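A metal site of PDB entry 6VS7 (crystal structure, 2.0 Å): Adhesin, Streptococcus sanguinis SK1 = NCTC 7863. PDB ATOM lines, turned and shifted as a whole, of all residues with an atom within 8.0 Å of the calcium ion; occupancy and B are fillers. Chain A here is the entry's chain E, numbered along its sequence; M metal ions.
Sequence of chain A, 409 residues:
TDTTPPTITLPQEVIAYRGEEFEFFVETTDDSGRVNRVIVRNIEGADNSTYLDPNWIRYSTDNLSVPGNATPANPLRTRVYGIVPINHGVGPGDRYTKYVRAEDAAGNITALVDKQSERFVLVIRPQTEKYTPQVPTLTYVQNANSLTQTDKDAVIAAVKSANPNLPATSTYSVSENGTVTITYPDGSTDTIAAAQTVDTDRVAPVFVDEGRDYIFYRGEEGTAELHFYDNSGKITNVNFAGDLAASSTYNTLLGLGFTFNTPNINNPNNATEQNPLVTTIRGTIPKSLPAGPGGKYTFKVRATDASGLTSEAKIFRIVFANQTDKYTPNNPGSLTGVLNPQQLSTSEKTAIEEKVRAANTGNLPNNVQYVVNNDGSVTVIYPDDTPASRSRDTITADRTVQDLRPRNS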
ATOM      1  N   THR A   1      22.838   1.139  23.805  1.00  0.00           N
ATOM      2  CA  THR A   1      23.649   2.181  24.368  1.00  0.00           C
ATOM      3  C   THR A   1      22.945   3.463  24.864  1.00  0.00           C
ATOM      4  O   THR A   1      23.491   4.217  25.661  1.00  0.00           O
ATOM      5  CB  THR A   1      24.846   2.514  23.494  1.00  0.00           C
ATOM      6  OG1 THR A   1      25.683   3.453  24.179  1.00  0.00           O
ATOM      7  CG2 THR A   1      24.404   3.068  22.174  1.00  0.00           C
ATOM      8  N   ASP A   2      21.754   3.709  24.457  1.00  0.00           N
ATOM      9  CA  ASP A   2      21.070   4.874  24.988  1.00  0.00           C
ATOM     10  C   ASP A   2      21.016   5.844  23.851  1.00  0.00           C
ATOM     11  O   ASP A   2      21.824   6.703  23.768  1.00  0.00           O
ATOM     12  CB  ASP A   2      21.095   5.606  26.321  1.00  0.00           C
ATOM     13  CG  ASP A   2      19.923   6.545  26.527  1.00  0.00           C
ATOM     14  OD1 ASP A   2      19.141   6.763  25.623  1.00  0.00           O
ATOM     15  OD2 ASP A   2      19.808   7.029  27.633  1.00  0.00           O
ATOM     16  N   THR A   3      20.193   5.518  22.859  1.00  0.00           N
ATOM     17  CA  THR A   3      19.984   6.367  21.690  1.00  0.00           C
ATOM     18  C   THR A   3      18.570   6.940  21.637  1.00  0.00           C
ATOM     19  O   THR A   3      18.076   7.270  20.553  1.00  0.00           O
ATOM     20  CB  THR A   3      20.268   5.608  20.395  1.00  0.00           C
ATOM     21  OG1 THR A   3      19.339   4.526  20.262  1.00  0.00           O
ATOM     22  CG2 THR A   3      21.684   5.077  20.374  1.00  0.00           C
ATOM     23  N   THR A   4      17.937   7.052  22.795  1.00  0.00           N
ATOM     24  CA  THR A   4      16.587   7.565  22.933  1.00  0.00           C
ATOM     25  C   THR A   4      16.431   8.805  23.744  1.00  0.00           C
ATOM     26  O   THR A   4      16.875   8.852  24.834  1.00  0.00           O
ATOM     27  CB  THR A   4      15.741   6.410  23.472  1.00  0.00           C
ATOM     28  OG1 THR A   4      15.743   5.419  22.490  1.00  0.00           O
ATOM     29  CG2 THR A   4      14.308   6.789  23.723  1.00  0.00           C
ATOM     30  N   PRO A   5      15.753   9.832  23.199  1.00  0.00           N
ATOM     31  CA  PRO A   5      15.705  11.077  23.985  1.00  0.00           C
ATOM     32  C   PRO A   5      14.679  10.997  25.093  1.00  0.00           C
ATOM     33  O   PRO A   5      13.818  10.098  25.108  1.00  0.00           O
ATOM     34  CB  PRO A   5      15.305  12.126  22.925  1.00  0.00           C
ATOM     35  CG  PRO A   5      14.557  11.338  21.891  1.00  0.00           C
ATOM     36  CD  PRO A   5      15.257  10.002  21.828  1.00  0.00           C
ATOM     37  N   PRO A   6      14.725  11.920  26.052  1.00  0.00           N
ATOM     38  CA  PRO A   6      13.769  11.882  27.154  1.00  0.00           C
ATOM     39  C   PRO A   6      12.333  12.061  26.688  1.00  0.00           C
ATOM     40  O   PRO A   6      12.055  12.500  25.569  1.00  0.00           O
ATOM     41  CB  PRO A   6      14.209  13.064  28.037  1.00  0.00           C
ATOM     42  CG  PRO A   6      15.643  13.325  27.625  1.00  0.00           C
ATOM     43  CD  PRO A   6      15.701  13.020  26.178  1.00  0.00           C
ATOM     44  N   THR A   7      11.398  11.687  27.534  1.00  0.00           N
ATOM     45  CA  THR A   7      10.000  11.773  27.293  1.00  0.00           C
ATOM     46  C   THR A   7       9.487  12.989  28.051  1.00  0.00           C
ATOM     47  O   THR A   7       9.604  13.051  29.238  1.00  0.00           O
ATOM     48  CB  THR A   7       9.322  10.497  27.832  1.00  0.00           C
ATOM     49  OG1 THR A   7       9.461   9.430  26.912  1.00  0.00           O
ATOM     50  CG2 THR A   7       7.929  10.696  28.113  1.00  0.00           C
ATOM     51  N   THR A  29      11.115  12.427  31.649  1.00  0.00           N
ATOM     52  CA  THR A  29      11.477  11.092  32.084  1.00  0.00           C
ATOM     53  C   THR A  29      12.445  10.483  31.081  1.00  0.00           C
ATOM     54  O   THR A  29      12.394  10.792  29.895  1.00  0.00           O
ATOM     55  CB  THR A  29      10.220  10.237  32.233  1.00  0.00           C
ATOM     56  OG1 THR A  29       9.944  10.045  33.627  1.00  0.00           O
ATOM     57  CG2 THR A  29      10.339   8.903  31.525  1.00  0.00           C
ATOM     58  N   ASP A  30      13.347   9.623  31.579  1.00  0.00           N
ATOM     59  CA  ASP A  30      14.298   8.974  30.699  1.00  0.00           C
ATOM     60  C   ASP A  30      14.644   7.584  31.224  1.00  0.00           C
ATOM     61  O   ASP A  30      14.737   7.374  32.431  1.00  0.00           O
ATOM     62  CB  ASP A  30      15.578   9.801  30.544  1.00  0.00           C
ATOM     63  CG  ASP A  30      16.439   9.311  29.401  1.00  0.00           C
ATOM     64  OD1 ASP A  30      16.122   9.646  28.241  1.00  0.00           O
ATOM     65  OD2 ASP A  30      17.442   8.582  29.665  1.00  0.00           O
ATOM     66  N   ASP A  31      14.850   6.640  30.301  1.00  0.00           N
ATOM     67  CA  ASP A  31      15.191   5.275  30.713  1.00  0.00           C
ATOM     68  C   ASP A  31      16.461   5.261  31.560  1.00  0.00           C
ATOM     69  O   ASP A  31      16.518   4.563  32.580  1.00  0.00           O
ATOM     70  CB  ASP A  31      15.322   4.365  29.487  1.00  0.00           C
ATOM     71  CG  ASP A  31      14.014   3.686  29.130  1.00  0.00           C
ATOM     72  OD1 ASP A  31      13.060   3.750  29.949  1.00  0.00           O
ATOM     73  OD2 ASP A  31      13.915   3.078  28.050  1.00  0.00           O
ATOM     74  N   SER A  32      17.476   6.040  31.176  1.00  0.00           N
ATOM     75  CA  SER A  32      18.690   6.169  31.973  1.00  0.00           C
ATOM     76  C   SER A  32      18.471   6.798  33.334  1.00  0.00           C
ATOM     77  O   SER A  32      19.435   6.880  34.103  1.00  0.00           O
ATOM     78  CB  SER A  32      19.700   7.030  31.207  1.00  0.00           C
ATOM     79  OG  SER A  32      19.339   8.399  31.368  1.00  0.00           O
ATOM     80  N   GLY A  33      17.282   7.287  33.639  1.00  0.00           N
ATOM     81  CA  GLY A  33      17.022   7.911  34.915  1.00  0.00           C
ATOM     82  C   GLY A  33      17.647   9.269  35.100  1.00  0.00           C
ATOM     83  O   GLY A  33      17.469   9.866  36.179  1.00  0.00           O
ATOM     84  N   ARG A  34      18.323   9.800  34.096  1.00  0.00           N
ATOM     85  CA  ARG A  34      19.026  11.077  34.220  1.00  0.00           C
ATOM     86  C   ARG A  34      18.819  11.947  32.979  1.00  0.00           C
ATOM     87  O   ARG A  34      19.027  11.507  31.846  1.00  0.00           O
ATOM     88  CB  ARG A  34      20.536  10.848  34.439  1.00  0.00           C
ATOM     89  CG  ARG A  34      21.350  12.114  34.253  1.00  0.00           C
ATOM     90  CD  ARG A  34      22.810  11.954  34.589  1.00  0.00           C
ATOM     91  NE  ARG A  34      23.584  13.146  34.263  1.00  0.00           N
ATOM     92  CZ  ARG A  34      24.854  13.352  34.623  1.00  0.00           C
ATOM     93  NH1 ARG A  34      25.506  12.435  35.333  1.00  0.00           N
ATOM     94  NH2 ARG A  34      25.475  14.459  34.288  1.00  0.00           N
ATOM     95  N   VAL A  35      18.397  13.201  33.218  1.00  0.00           N
ATOM     96  CA  VAL A  35      18.263  14.220  32.180  1.00  0.00           C
ATOM     97  C   VAL A  35      19.194  15.373  32.524  1.00  0.00           C
ATOM     98  O   VAL A  35      19.210  15.829  33.671  1.00  0.00           O
ATOM     99  CB  VAL A  35      16.809  14.713  32.060  1.00  0.00           C
ATOM    100  CG1 VAL A  35      16.733  15.948  31.149  1.00  0.00           C
ATOM    101  CG2 VAL A  35      15.908  13.611  31.514  1.00  0.00           C
ATOM    102  N   GLU A 103      17.300  16.779  27.061  1.00  0.00           N
ATOM    103  CA  GLU A 103      18.450  16.035  26.573  1.00  0.00           C
ATOM    104  C   GLU A 103      19.014  15.181  27.699  1.00  0.00           C
ATOM    105  O   GLU A 103      19.150  15.667  28.837  1.00  0.00           O
ATOM    106  CB  GLU A 103      19.516  16.997  26.026  1.00  0.00           C
ATOM    107  CG  GLU A 103      20.734  16.305  25.410  1.00  0.00           C
ATOM    108  CD  GLU A 103      21.787  17.319  24.983  1.00  0.00           C
ATOM    109  OE1 GLU A 103      22.979  16.951  24.896  1.00  0.00           O
ATOM    110  OE2 GLU A 103      21.416  18.489  24.735  1.00  0.00           O
ATOM    111  N   ASP A 104      19.317  13.909  27.406  1.00  0.00           N
ATOM    112  CA  ASP A 104      19.762  12.995  28.460  1.00  0.00           C
ATOM    113  C   ASP A 104      21.288  13.110  28.612  1.00  0.00           C
ATOM    114  O   ASP A 104      21.932  13.943  27.968  1.00  0.00           O
ATOM    115  CB  ASP A 104      19.294  11.563  28.168  1.00  0.00           C
ATOM    116  CG  ASP A 104      19.900  10.969  26.913  1.00  0.00           C
ATOM    117  OD1 ASP A 104      20.876  11.537  26.366  1.00  0.00           O
ATOM    118  OD2 ASP A 104      19.387   9.910  26.464  1.00  0.00           O
ATOM    119  N   ALA A 105      21.876  12.250  29.454  1.00  0.00           N
ATOM    120  CA  ALA A 105      23.323  12.301  29.656  1.00  0.00           C
ATOM    121  C   ALA A 105      24.085  11.856  28.419  1.00  0.00           C
ATOM    122  O   ALA A 105      25.187  12.363  28.164  1.00  0.00           O
ATOM    123  CB  ALA A 105      23.729  11.471  30.881  1.00  0.00           C
ATOM    124  N   ALA A 106      23.527  10.929  27.641  1.00  0.00           N
ATOM    125  CA  ALA A 106      24.181  10.452  26.420  1.00  0.00           C
ATOM    126  C   ALA A 106      24.054  11.421  25.247  1.00  0.00           C
ATOM    127  O   ALA A 106      24.559  11.116  24.165  1.00  0.00           O
ATOM    128  CB  ALA A 106      23.607   9.091  26.016  1.00  0.00           C
ATOM    129  N   GLY A 107      23.416  12.579  25.437  1.00  0.00           N
ATOM    130  CA  GLY A 107      23.337  13.558  24.354  1.00  0.00           C
ATOM    131  C   GLY A 107      22.176  13.377  23.416  1.00  0.00           C
ATOM    132  O   GLY A 107      22.185  13.920  22.309  1.00  0.00           O
ATOM    133  N   ASN A 108      21.151  12.627  23.828  1.00  0.00           N
ATOM    134  CA  ASN A 108      19.947  12.468  23.028  1.00  0.00           C
ATOM    135  C   ASN A 108      18.991  13.612  23.382  1.00  0.00           C
ATOM    136  O   ASN A 108      18.476  13.674  24.513  1.00  0.00           O
ATOM    137  CB  ASN A 108      19.310  11.107  23.301  1.00  0.00           C
ATOM    138  CG  ASN A 108      20.287   9.955  23.081  1.00  0.00           C
ATOM    139  OD1 ASN A 108      20.902   9.854  22.030  1.00  0.00           O
ATOM    140  ND2 ASN A 108      20.407   9.081  24.086  1.00  0.00           N
ATOM    141  N   ILE A 109      18.792  14.544  22.440  1.00  0.00           N
ATOM    142  CA  ILE A 109      17.871  15.665  22.603  1.00  0.00           C
ATOM    143  C   ILE A 109      16.605  15.374  21.810  1.00  0.00           C
ATOM    144  O   ILE A 109      16.631  14.710  20.769  1.00  0.00           O
ATOM    145  CB  ILE A 109      18.544  16.980  22.141  1.00  0.00           C
ATOM    146  CG1 ILE A 109      17.685  18.201  22.516  1.00  0.00           C
ATOM    147  CG2 ILE A 109      18.805  16.980  20.634  1.00  0.00           C
ATOM    148  CD1 ILE A 109      18.439  19.530  22.382  1.00  0.00           C
HETATM  149 CA    CA M   1      17.622   8.199  27.034  1.00  0.00          CA
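OG of Ser 32 lies close to OD2 of Asp 30, at 2.6 Å.
The backbone NH (N) of Thr 4 sits close to the side-chain amide nitrogen (ND2) of Asn 108, 3.4 Å away.
The backbone carbonyl oxygen (O) of Asp 2 sits at hydrogen-bond distance from the side-chain amide nitrogen (ND2) of Asn 108 (2.8 Å).
The side-chain carboxylate (OD1) of Asp 104 lies within hydrogen-bond range of the backbone NH (N) of Asn 108 (2.8 Å).
OD1 of Asp 104 lies within hydrogen-bond range of N of Gly 107 (2.9 Å).
The side-chain carboxylate of Asp 104 is in hydrogen-bond range of the backbone NH of Ala 106.
Of the 21 residues printed, 4 come within 4 Å of the calcium ion.
Along chain A the residues within 4 Å of the calcium ion span positions 2 to 104.
The nearest printed residue that does not touch the calcium ion is Asn 108 (4.2 Å).
The calcium ion is bound by OD1 of Asp 30, O of Thr 4, OD1 of Asp 2, OD2 of Asp 104, OD2 of Asp 2 and OD2 of Asp 30.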
